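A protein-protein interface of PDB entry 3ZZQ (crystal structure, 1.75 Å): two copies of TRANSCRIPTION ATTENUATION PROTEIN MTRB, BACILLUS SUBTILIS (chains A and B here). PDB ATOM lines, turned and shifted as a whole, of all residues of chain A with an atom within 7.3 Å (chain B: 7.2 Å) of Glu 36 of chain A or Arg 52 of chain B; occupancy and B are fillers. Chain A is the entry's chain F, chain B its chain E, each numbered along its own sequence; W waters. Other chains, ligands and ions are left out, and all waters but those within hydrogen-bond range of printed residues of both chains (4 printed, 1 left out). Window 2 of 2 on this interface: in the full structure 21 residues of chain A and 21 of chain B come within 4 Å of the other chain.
Water W3 lies within hydrogen-bond range of the side-chain carboxylate (OE1) of Glu 36 of chain A (2.7 Å), the guanidinium group (NH1) of Arg 52 of chain B (2.7 Å), the backbone carbonyl oxygen (O) of Lys 31 of chain A (2.9 Å) and the side-chain amino group (NZ) of Lys 50 of chain B (3.4 Å).
Water W2 lies within hydrogen-bond range of the side-chain amino group (NZ) of Lys 7 of chain A and the backbone carbonyl oxygen (O) of Ala 55 of chain B.
Water W1 lies within hydrogen-bond range of the side-chain carboxylate of Glu 36 of chain A (2.9 Å) and the backbone NH of Gly 53 of chain B (3.3 Å).
Water W4 lies within hydrogen-bond range of O of Lys 34 of chain A (3.2 Å) and N of Gly 53 of chain B (3.4 Å).
OE2 of Glu 30 of chain A touches CE1 of Phe 26 of chain B (3.4 Å).
CD2 of Leu 32 of chain A touches CE of Lys 50 of chain B, 3.6 Å away.
Glu 36 of chain A touches Val 51 of chain B (CA to O, 3.5 Å).
Lys 50 of chain B touches Val 37 of chain A (CA to O, 3.4 Å).
Val 37 of chain A touches Ile 57 of chain B (CG2 to CD1, 3.6 Å).
The side-chain amino group (NZ) of Lys 50 of chain B is in salt-bridge range of the side-chain carboxylate (OE1) of Glu 30 of chain A.
The backbone carbonyl oxygen of Lys 31 of chain A lies within hydrogen-bond range of the side-chain amino group of Lys 50 of chain B (2.8 Å).
The backbone NH of Val 51 of chain B sits at hydrogen-bond distance from the backbone carbonyl oxygen of Val 37 of chain A (2.8 Å).
The side-chain carboxylate of Glu 36 of chain A lies within salt-bridge range of the guanidinium group of Arg 52 of chain B.
Of the printed residues of chain B, Glu 30 of chain A touches Phe 26 (3.4 Å) and Lys 50 (2.9 Å).
Of the printed residues of chain B, Lys 31 of chain A touches Lys 50.
Printed residues of chain B within 4 Å of Val 37 of chain A: Lys 50, Val 51 and Ile 57.
Ile 6 of chain B touches none of the printed residues of chain A.
The nearest residue of chain B that does not touch Glu 36 of chain A is Lys 50 of chain B (4.4 Å).
The backbone NH (N) of Asn 14 of chain B is in hydrogen-bond range of the backbone carbonyl oxygen (O) of Arg 52 of chain B (2.9 Å).
The backbone NH of Ile 16 of chain B sits at hydrogen-bond distance from the backbone carbonyl oxygen of Lys 50 of chain B, 2.8 Å away.
O of Glu 36 of chain A lies within hydrogen-bond range of N of Ala 8 of chain A.
N of Leu 32 of chain A is in hydrogen-bond range of O of Val 13 of chain A.
N of Asp 33 of chain A sits at hydrogen-bond distance from OE1 of Glu 36 of chain A (2.8 Å).
5 positions are printed for both chains.
Of the 17 printed residues of chain A, 5 touch a printed residue of chain B.
Hydrophobic or aromatic side chains of chain A within 4 Å of the printed part of chain B: Leu 32 and Val 37.
Hydrophobic or aromatic side chains of chain B within 4 Å of the printed part of chain A: Phe 26 and Ile 57.
Among the printed residues, Asp or Glu carboxylates within 4 Å of a Lys or Arg side-chain nitrogen of the other chain: Glu 30 of chain A with Lys 50 of chain B (2.9 Å) and Glu 36 of chain A with Arg 52 of chain B (2.9 Å).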
ATOM      1  N   ILE A   6     -23.121  -0.201   6.652  1.00  0.00           N
ATOM      2  CA  ILE A   6     -24.085  -1.301   6.561  1.00  0.00           C
ATOM      3  C   ILE A   6     -23.866  -2.271   7.720  1.00  0.00           C
ATOM      4  O   ILE A   6     -22.782  -2.847   7.861  1.00  0.00           O
ATOM      5  CB  ILE A   6     -23.951  -2.051   5.207  1.00  0.00           C
ATOM      6  CG1 ILE A   6     -24.156  -1.081   4.040  1.00  0.00           C
ATOM      7  CG2 ILE A   6     -24.957  -3.218   5.134  1.00  0.00           C
ATOM      8  CD1 ILE A   6     -23.464  -1.474   2.745  1.00  0.00           C
ATOM      9  N   LYS A   7     -24.889  -2.440   8.559  1.00  0.00           N
ATOM     10  CA  LYS A   7     -24.835  -3.389   9.672  1.00  0.00           C
ATOM     11  C   LYS A   7     -25.897  -4.466   9.469  1.00  0.00           C
ATOM     12  O   LYS A   7     -27.057  -4.148   9.223  1.00  0.00           O
ATOM     13  CB  LYS A   7     -25.056  -2.677  11.012  1.00  0.00           C
ATOM     14  CG  LYS A   7     -25.006  -3.595  12.219  1.00  0.00           C
ATOM     15  CD  LYS A   7     -24.883  -2.814  13.524  1.00  0.00           C
ATOM     16  CE  LYS A   7     -24.791  -3.755  14.713  1.00  0.00           C
ATOM     17  NZ  LYS A   7     -24.438  -3.045  15.971  1.00  0.00           N
ATOM     18  N   ALA A   8     -25.497  -5.728   9.564  1.00  0.00           N
ATOM     19  CA  ALA A   8     -26.432  -6.843   9.410  1.00  0.00           C
ATOM     20  C   ALA A   8     -27.296  -6.959  10.669  1.00  0.00           C
ATOM     21  O   ALA A   8     -26.767  -6.996  11.782  1.00  0.00           O
ATOM     22  CB  ALA A   8     -25.682  -8.133   9.177  1.00  0.00           C
ATOM     23  N   VAL A   9     -28.613  -6.989  10.478  1.00  0.00           N
ATOM     24  CA  VAL A   9     -29.574  -7.198  11.572  1.00  0.00           C
ATOM     25  C   VAL A   9     -29.894  -8.694  11.703  1.00  0.00           C
ATOM     26  O   VAL A   9     -30.410  -9.143  12.733  1.00  0.00           O
ATOM     27  CB  VAL A   9     -30.884  -6.409  11.333  1.00  0.00           C
ATOM     28  CG1 VAL A   9     -31.847  -6.576  12.517  1.00  0.00           C
ATOM     29  CG2 VAL A   9     -30.593  -4.935  11.101  1.00  0.00           C
ATOM     30  N   GLU A  10     -29.582  -9.454  10.658  1.00  0.00           N
ATOM     31  CA  GLU A  10     -29.748 -10.902  10.642  1.00  0.00           C
ATOM     32  C   GLU A  10     -28.524 -11.529   9.985  1.00  0.00           C
ATOM     33  O   GLU A  10     -27.732 -10.834   9.356  1.00  0.00           O
ATOM     34  CB  GLU A  10     -31.000 -11.276   9.844  1.00  0.00           C
ATOM     35  CG  GLU A  10     -30.930 -10.877   8.361  1.00  0.00           C
ATOM     36  CD  GLU A  10     -32.160 -11.276   7.561  1.00  0.00           C
ATOM     37  OE1 GLU A  10     -33.054 -11.953   8.115  1.00  0.00           O
ATOM     38  OE2 GLU A  10     -32.226 -10.914   6.366  1.00  0.00           O
ATOM     39  N   ASP A  11     -28.383 -12.842  10.101  1.00  0.00           N
ATOM     40  CA  ASP A  11     -27.298 -13.535   9.409  1.00  0.00           C
ATOM     41  C   ASP A  11     -27.515 -13.543   7.899  1.00  0.00           C
ATOM     42  O   ASP A  11     -28.649 -13.484   7.418  1.00  0.00           O
ATOM     43  CB  ASP A  11     -27.184 -14.984   9.883  1.00  0.00           C
ATOM     44  CG  ASP A  11     -26.665 -15.103  11.299  1.00  0.00           C
ATOM     45  OD1 ASP A  11     -25.975 -14.182  11.791  1.00  0.00           O
ATOM     46  OD2 ASP A  11     -26.943 -16.148  11.917  1.00  0.00           O
ATOM     47  N   VAL A  13     -26.476 -11.483   5.343  1.00  0.00           N
ATOM     48  CA  VAL A  13     -26.590 -10.260   4.540  1.00  0.00           C
ATOM     49  C   VAL A  13     -25.435 -10.226   3.545  1.00  0.00           C
ATOM     50  O   VAL A  13     -24.309 -10.522   3.918  1.00  0.00           O
ATOM     51  CB  VAL A  13     -26.533  -9.002   5.432  1.00  0.00           C
ATOM     52  CG1 VAL A  13     -26.464  -7.720   4.586  1.00  0.00           C
ATOM     53  CG2 VAL A  13     -27.731  -8.961   6.354  1.00  0.00           C
ATOM     54  N   GLU A  30     -19.451  -9.225  -0.080  1.00  0.00           N
ATOM     55  CA  GLU A  30     -19.056  -9.512   1.287  1.00  0.00           C
ATOM     56  C   GLU A  30     -20.273  -9.986   2.037  1.00  0.00           C
ATOM     57  O   GLU A  30     -21.349  -9.394   1.935  1.00  0.00           O
ATOM     58  CB  GLU A  30     -18.518  -8.268   1.987  1.00  0.00           C
ATOM     59  CG  GLU A  30     -17.103  -7.939   1.641  1.00  0.00           C
ATOM     60  CD  GLU A  30     -16.108  -9.000   2.063  1.00  0.00           C
ATOM     61  OE1 GLU A  30     -16.345  -9.753   3.051  1.00  0.00           O
ATOM     62  OE2 GLU A  30     -15.074  -9.084   1.382  1.00  0.00           O
ATOM     63  N   LYS A  31     -20.105 -11.056   2.798  1.00  0.00           N
ATOM     64  CA  LYS A  31     -21.186 -11.568   3.603  1.00  0.00           C
ATOM     65  C   LYS A  31     -21.032 -11.035   5.026  1.00  0.00           C
ATOM     66  O   LYS A  31     -19.924 -11.024   5.568  1.00  0.00           O
ATOM     67  CB  LYS A  31     -21.162 -13.085   3.590  1.00  0.00           C
ATOM     68  CG  LYS A  31     -22.323 -13.722   4.307  1.00  0.00           C
ATOM     69  CD  LYS A  31     -22.334 -15.201   4.020  1.00  0.00           C
ATOM     70  CE  LYS A  31     -23.098 -15.976   5.058  1.00  0.00           C
ATOM     71  NZ  LYS A  31     -22.682 -17.405   5.048  1.00  0.00           N
ATOM     72  N   LEU A  32     -22.139 -10.579   5.609  1.00  0.00           N
ATOM     73  CA  LEU A  32     -22.166 -10.130   6.995  1.00  0.00           C
ATOM     74  C   LEU A  32     -23.116 -11.020   7.776  1.00  0.00           C
ATOM     75  O   LEU A  32     -24.255 -11.235   7.362  1.00  0.00           O
ATOM     76  CB  LEU A  32     -22.661  -8.688   7.108  1.00  0.00           C
ATOM     77  CG  LEU A  32     -21.852  -7.586   6.428  1.00  0.00           C
ATOM     78  CD1 LEU A  32     -22.590  -6.262   6.538  1.00  0.00           C
ATOM     79  CD2 LEU A  32     -20.480  -7.472   7.037  1.00  0.00           C
ATOM     80  N   ASP A  33     -22.645 -11.536   8.903  1.00  0.00           N
ATOM     81  CA  ASP A  33     -23.532 -12.190   9.846  1.00  0.00           C
ATOM     82  C   ASP A  33     -24.033 -11.162  10.855  1.00  0.00           C
ATOM     83  O   ASP A  33     -23.568 -10.021  10.873  1.00  0.00           O
ATOM     84  CB  ASP A  33     -22.838 -13.386  10.501  1.00  0.00           C
ATOM     85  CG  ASP A  33     -22.793 -14.603   9.578  1.00  0.00           C
ATOM     86  OD1 ASP A  33     -23.660 -14.711   8.675  1.00  0.00           O
ATOM     87  OD2 ASP A  33     -21.893 -15.450   9.750  1.00  0.00           O
ATOM     88  N   LYS A  34     -25.007 -11.552  11.668  1.00  0.00           N
ATOM     89  CA  LYS A  34     -25.678 -10.614  12.566  1.00  0.00           C
ATOM     90  C   LYS A  34     -24.686  -9.781  13.379  1.00  0.00           C
ATOM     91  O   LYS A  34     -23.781 -10.324  14.006  1.00  0.00           O
ATOM     92  CB  LYS A  34     -26.625 -11.371  13.511  1.00  0.00           C
ATOM     93  CG  LYS A  34     -27.518 -10.464  14.335  1.00  0.00           C
ATOM     94  CD  LYS A  34     -28.593 -11.257  15.073  1.00  0.00           C
ATOM     95  CE  LYS A  34     -29.391 -10.354  16.003  1.00  0.00           C
ATOM     96  NZ  LYS A  34     -30.478 -11.096  16.711  1.00  0.00           N
ATOM     97  N   GLY A  35     -24.846  -8.457  13.336  1.00  0.00           N
ATOM     98  CA  GLY A  35     -24.016  -7.547  14.119  1.00  0.00           C
ATOM     99  C   GLY A  35     -22.768  -7.037  13.411  1.00  0.00           C
ATOM    100  O   GLY A  35     -22.168  -6.054  13.844  1.00  0.00           O
ATOM    101  N   GLU A  36     -22.375  -7.702  12.328  1.00  0.00           N
ATOM    102  CA  GLU A  36     -21.171  -7.331  11.580  1.00  0.00           C
ATOM    103  C   GLU A  36     -21.452  -6.122  10.704  1.00  0.00           C
ATOM    104  O   GLU A  36     -22.578  -5.910  10.274  1.00  0.00           O
ATOM    105  CB  GLU A  36     -20.680  -8.501  10.734  1.00  0.00           C
ATOM    106  CG  GLU A  36     -20.284  -9.688  11.587  1.00  0.00           C
ATOM    107  CD  GLU A  36     -19.660 -10.826  10.807  1.00  0.00           C
ATOM    108  OE1 GLU A  36     -19.977 -11.006   9.613  1.00  0.00           O
ATOM    109  OE2 GLU A  36     -18.848 -11.556  11.410  1.00  0.00           O
ATOM    110  N   VAL A  37     -20.410  -5.334  10.450  1.00  0.00           N
ATOM    111  CA  VAL A  37     -20.548  -4.048   9.785  1.00  0.00           C
ATOM    112  C   VAL A  37     -19.543  -3.941   8.645  1.00  0.00           C
ATOM    113  O   VAL A  37     -18.411  -4.415   8.765  1.00  0.00           O
ATOM    114  CB  VAL A  37     -20.302  -2.886  10.783  1.00  0.00           C
ATOM    115  CG1 VAL A  37     -20.333  -1.532  10.071  1.00  0.00           C
ATOM    116  CG2 VAL A  37     -21.318  -2.926  11.918  1.00  0.00           C
ATOM    117  N   ILE A  38     -19.965  -3.336   7.542  1.00  0.00           N
ATOM    118  CA  ILE A  38     -19.026  -2.875   6.519  1.00  0.00           C
ATOM    119  C   ILE A  38     -19.231  -1.381   6.286  1.00  0.00           C
ATOM    120  O   ILE A  38     -20.365  -0.896   6.227  1.00  0.00           O
ATOM    121  CB  ILE A  38     -19.102  -3.696   5.207  1.00  0.00           C
ATOM    122  CG1 ILE A  38     -17.989  -3.259   4.239  1.00  0.00           C
ATOM    123  CG2 ILE A  38     -20.468  -3.585   4.549  1.00  0.00           C
ATOM    124  CD1 ILE A  38     -17.537  -4.367   3.277  1.00  0.00           C
ATOM    125  N   LEU A  56     -29.205  -2.539   8.671  1.00  0.00           N
ATOM    126  CA  LEU A  56     -29.327  -1.143   9.049  1.00  0.00           C
ATOM    127  C   LEU A  56     -28.308  -0.382   8.208  1.00  0.00           C
ATOM    128  O   LEU A  56     -27.128  -0.739   8.187  1.00  0.00           O
ATOM    129  CB  LEU A  56     -29.019  -0.982  10.531  1.00  0.00           C
ATOM    130  CG  LEU A  56     -29.031   0.434  11.108  1.00  0.00           C
ATOM    131  CD1 LEU A  56     -30.434   1.015  11.055  1.00  0.00           C
ATOM    132  CD2 LEU A  56     -28.499   0.412  12.536  1.00  0.00           C
ATOM    133  N   ILE B   6     -13.772   2.847  15.910  1.00  0.00           N
ATOM    134  CA  ILE B   6     -14.292   1.536  16.300  1.00  0.00           C
ATOM    135  C   ILE B   6     -13.808   1.215  17.707  1.00  0.00           C
ATOM    136  O   ILE B   6     -12.600   1.206  17.963  1.00  0.00           O
ATOM    137  CB  ILE B   6     -13.821   0.438  15.326  1.00  0.00           C
ATOM    138  CG1 ILE B   6     -14.286   0.740  13.903  1.00  0.00           C
ATOM    139  CG2 ILE B   6     -14.325  -0.943  15.784  1.00  0.00           C
ATOM    140  CD1 ILE B   6     -13.306   0.327  12.827  1.00  0.00           C
ATOM    141  N   ASP B  11     -14.156  -8.782  23.904  1.00  0.00           N
ATOM    142  CA  ASP B  11     -12.939  -9.331  23.306  1.00  0.00           C
ATOM    143  C   ASP B  11     -13.241  -9.963  21.946  1.00  0.00           C
ATOM    144  O   ASP B  11     -14.357 -10.417  21.693  1.00  0.00           O
ATOM    145  CB  ASP B  11     -12.306 -10.402  24.208  1.00  0.00           C
ATOM    146  CG  ASP B  11     -11.684  -9.834  25.471  1.00  0.00           C
ATOM    147  OD1 ASP B  11     -11.446  -8.613  25.556  1.00  0.00           O
ATOM    148  OD2 ASP B  11     -11.411 -10.634  26.395  1.00  0.00           O
ATOM    149  N   GLY B  12     -12.233  -9.989  21.079  1.00  0.00           N
ATOM    150  CA  GLY B  12     -12.310 -10.722  19.819  1.00  0.00           C
ATOM    151  C   GLY B  12     -12.906  -9.960  18.648  1.00  0.00           C
ATOM    152  O   GLY B  12     -13.356 -10.569  17.676  1.00  0.00           O
ATOM    153  N   VAL B  13     -12.922  -8.631  18.733  1.00  0.00           N
ATOM    154  CA  VAL B  13     -13.332  -7.808  17.592  1.00  0.00           C
ATOM    155  C   VAL B  13     -12.198  -7.777  16.569  1.00  0.00           C
ATOM    156  O   VAL B  13     -11.031  -7.697  16.944  1.00  0.00           O
ATOM    157  CB  VAL B  13     -13.700  -6.375  18.024  1.00  0.00           C
ATOM    158  CG1 VAL B  13     -13.948  -5.469  16.797  1.00  0.00           C
ATOM    159  CG2 VAL B  13     -14.923  -6.394  18.919  1.00  0.00           C
ATOM    160  N   ASN B  14     -12.543  -7.862  15.287  1.00  0.00           N
ATOM    161  CA  ASN B  14     -11.569  -7.730  14.209  1.00  0.00           C
ATOM    162  C   ASN B  14     -11.963  -6.592  13.288  1.00  0.00           C
ATOM    163  O   ASN B  14     -13.120  -6.503  12.881  1.00  0.00           O
ATOM    164  CB  ASN B  14     -11.452  -9.025  13.406  1.00  0.00           C
ATOM    165  CG  ASN B  14     -10.451  -9.992  14.006  1.00  0.00           C
ATOM    166  OD1 ASN B  14      -9.242  -9.852  13.814  1.00  0.00           O
ATOM    167  ND2 ASN B  14     -10.946 -10.973  14.735  1.00  0.00           N
ATOM    168  N   VAL B  15     -10.998  -5.730  12.983  1.00  0.00           N
ATOM    169  CA  VAL B  15     -11.179  -4.634  12.046  1.00  0.00           C
ATOM    170  C   VAL B  15     -10.329  -4.952  10.822  1.00  0.00           C
ATOM    171  O   VAL B  15      -9.106  -5.057  10.919  1.00  0.00           O
ATOM    172  CB  VAL B  15     -10.741  -3.283  12.654  1.00  0.00           C
ATOM    173  CG1 VAL B  15     -10.876  -2.155  11.616  1.00  0.00           C
ATOM    174  CG2 VAL B  15     -11.577  -2.966  13.901  1.00  0.00           C
ATOM    175  N   ILE B  16     -10.984  -5.082   9.672  1.00  0.00           N
ATOM    176  CA  ILE B  16     -10.358  -5.619   8.474  1.00  0.00           C
ATOM    177  C   ILE B  16     -10.369  -4.597   7.347  1.00  0.00           C
ATOM    178  O   ILE B  16     -11.412  -4.047   7.018  1.00  0.00           O
ATOM    179  CB  ILE B  16     -11.119  -6.874   7.980  1.00  0.00           C
ATOM    180  CG1 ILE B  16     -11.263  -7.896   9.106  1.00  0.00           C
ATOM    181  CG2 ILE B  16     -10.407  -7.498   6.780  1.00  0.00           C
ATOM    182  CD1 ILE B  16     -12.227  -9.022   8.788  1.00  0.00           C
ATOM    183  N   PHE B  26      -8.706  -8.942   1.643  1.00  0.00           N
ATOM    184  CA  PHE B  26      -8.344  -8.468   2.970  1.00  0.00           C
ATOM    185  C   PHE B  26      -6.833  -8.286   3.012  1.00  0.00           C
ATOM    186  O   PHE B  26      -6.091  -9.240   2.766  1.00  0.00           O
ATOM    187  CB  PHE B  26      -8.743  -9.470   4.057  1.00  0.00           C
ATOM    188  CG  PHE B  26     -10.226  -9.740   4.167  1.00  0.00           C
ATOM    189  CD1 PHE B  26     -11.177  -8.971   3.502  1.00  0.00           C
ATOM    190  CD2 PHE B  26     -10.669 -10.764   4.996  1.00  0.00           C
ATOM    191  CE1 PHE B  26     -12.529  -9.248   3.641  1.00  0.00           C
ATOM    192  CE2 PHE B  26     -12.019 -11.039   5.131  1.00  0.00           C
ATOM    193  CZ  PHE B  26     -12.946 -10.282   4.454  1.00  0.00           C
ATOM    194  N   GLU B  30      -6.909  -6.217  12.179  1.00  0.00           N
ATOM    195  CA  GLU B  30      -6.455  -5.791  13.497  1.00  0.00           C
ATOM    196  C   GLU B  30      -7.399  -6.314  14.565  1.00  0.00           C
ATOM    197  O   GLU B  30      -8.601  -6.083  14.507  1.00  0.00           O
ATOM    198  CB  GLU B  30      -6.374  -4.271  13.564  1.00  0.00           C
ATOM    199  CG  GLU B  30      -5.634  -3.722  14.771  1.00  0.00           C
ATOM    200  CD  GLU B  30      -4.157  -4.088  14.805  1.00  0.00           C
ATOM    201  OE1 GLU B  30      -3.487  -4.108  13.745  1.00  0.00           O
ATOM    202  OE2 GLU B  30      -3.649  -4.337  15.919  1.00  0.00           O
ATOM    203  N   LEU B  32      -8.954  -6.356  18.281  1.00  0.00           N
ATOM    204  CA  LEU B  32      -9.206  -5.438  19.380  1.00  0.00           C
ATOM    205  C   LEU B  32      -9.787  -6.221  20.537  1.00  0.00           C
ATOM    206  O   LEU B  32     -10.789  -6.910  20.377  1.00  0.00           O
ATOM    207  CB  LEU B  32     -10.217  -4.366  18.988  1.00  0.00           C
ATOM    208  CG  LEU B  32      -9.843  -3.291  17.978  1.00  0.00           C
ATOM    209  CD1 LEU B  32     -10.993  -2.290  17.885  1.00  0.00           C
ATOM    210  CD2 LEU B  32      -8.559  -2.588  18.356  1.00  0.00           C
ATOM    211  N   LYS B  50     -14.256  -3.726   7.219  1.00  0.00           N
ATOM    212  CA  LYS B  50     -15.212  -4.676   7.771  1.00  0.00           C
ATOM    213  C   LYS B  50     -14.925  -4.833   9.255  1.00  0.00           C
ATOM    214  O   LYS B  50     -13.768  -4.905   9.654  1.00  0.00           O
ATOM    215  CB  LYS B  50     -15.099  -6.021   7.051  1.00  0.00           C
ATOM    216  CG  LYS B  50     -16.171  -7.042   7.425  1.00  0.00           C
ATOM    217  CD  LYS B  50     -16.103  -8.247   6.484  1.00  0.00           C
ATOM    218  CE  LYS B  50     -17.309  -9.163   6.632  1.00  0.00           C
ATOM    219  NZ  LYS B  50     -17.222 -10.358   5.727  1.00  0.00           N
ATOM    220  N   VAL B  51     -15.978  -4.860  10.061  1.00  0.00           N
ATOM    221  CA  VAL B  51     -15.844  -5.015  11.500  1.00  0.00           C
ATOM    222  C   VAL B  51     -16.650  -6.233  11.941  1.00  0.00           C
ATOM    223  O   VAL B  51     -17.854  -6.302  11.706  1.00  0.00           O
ATOM    224  CB  VAL B  51     -16.340  -3.783  12.256  1.00  0.00           C
ATOM    225  CG1 VAL B  51     -16.090  -3.947  13.747  1.00  0.00           C
ATOM    226  CG2 VAL B  51     -15.649  -2.525  11.741  1.00  0.00           C
ATOM    227  N   ARG B  52     -15.963  -7.182  12.570  1.00  0.00           N
ATOM    228  CA  ARG B  52     -16.584  -8.391  13.096  1.00  0.00           C
ATOM    229  C   ARG B  52     -16.489  -8.353  14.616  1.00  0.00           C
ATOM    230  O   ARG B  52     -15.475  -7.934  15.163  1.00  0.00           O
ATOM    231  CB  ARG B  52     -15.872  -9.629  12.548  1.00  0.00           C
ATOM    232  CG  ARG B  52     -15.889  -9.736  11.023  1.00  0.00           C
ATOM    233  CD  ARG B  52     -15.273 -11.046  10.536  1.00  0.00           C
ATOM    234  NE  ARG B  52     -16.076 -12.214  10.925  1.00  0.00           N
ATOM    235  CZ  ARG B  52     -16.567 -13.142  10.094  1.00  0.00           C
ATOM    236  NH1 ARG B  52     -16.347 -13.094   8.783  1.00  0.00           N
ATOM    237  NH2 ARG B  52     -17.287 -14.146  10.589  1.00  0.00           N
ATOM    238  N   GLY B  53     -17.549  -8.779  15.297  1.00  0.00           N
ATOM    239  CA  GLY B  53     -17.572  -8.785  16.758  1.00  0.00           C
ATOM    240  C   GLY B  53     -18.368  -7.607  17.270  1.00  0.00           C
ATOM    241  O   GLY B  53     -18.704  -6.704  16.509  1.00  0.00           O
ATOM    242  N   GLU B  54     -18.665  -7.598  18.562  1.00  0.00           N
ATOM    243  CA  GLU B  54     -19.511  -6.550  19.113  1.00  0.00           C
ATOM    244  C   GLU B  54     -18.681  -5.278  19.306  1.00  0.00           C
ATOM    245  O   GLU B  54     -17.757  -5.239  20.120  1.00  0.00           O
ATOM    246  CB  GLU B  54     -20.171  -7.008  20.415  1.00  0.00           C
ATOM    247  CG  GLU B  54     -21.491  -6.297  20.710  1.00  0.00           C
ATOM    248  CD  GLU B  54     -22.101  -6.683  22.055  1.00  0.00           C
ATOM    249  OE1 GLU B  54     -21.577  -7.600  22.728  1.00  0.00           O
ATOM    250  OE2 GLU B  54     -23.117  -6.060  22.437  1.00  0.00           O
ATOM    251  N   ALA B  55     -19.018  -4.249  18.535  1.00  0.00           N
ATOM    252  CA  ALA B  55     -18.260  -3.009  18.514  1.00  0.00           C
ATOM    253  C   ALA B  55     -19.183  -1.799  18.493  1.00  0.00           C
ATOM    254  O   ALA B  55     -20.326  -1.878  18.029  1.00  0.00           O
ATOM    255  CB  ALA B  55     -17.323  -2.988  17.300  1.00  0.00           C
ATOM    256  N   ILE B  57     -19.394   1.845  16.838  1.00  0.00           N
ATOM    257  CA  ILE B  57     -18.808   2.481  15.660  1.00  0.00           C
ATOM    258  C   ILE B  57     -19.339   3.892  15.480  1.00  0.00           C
ATOM    259  O   ILE B  57     -20.549   4.125  15.564  1.00  0.00           O
ATOM    260  CB  ILE B  57     -19.080   1.653  14.397  1.00  0.00           C
ATOM    261  CG1 ILE B  57     -18.403   0.282  14.515  1.00  0.00           C
ATOM    262  CG2 ILE B  57     -18.597   2.390  13.136  1.00  0.00           C
ATOM    263  CD1 ILE B  57     -18.890  -0.722  13.507  1.00  0.00           C
HETATM  264  O   HOH W   1     -19.227 -11.417  14.332  1.00  0.00           O
HETATM  265  O   HOH W   2     -22.186  -1.301  15.584  1.00  0.00           O
HETATM  266  O   HOH W   3     -18.806 -12.549   7.752  1.00  0.00           O
HETATM  267  O   HOH W   4     -20.896  -9.464  15.026  1.00  0.00           O
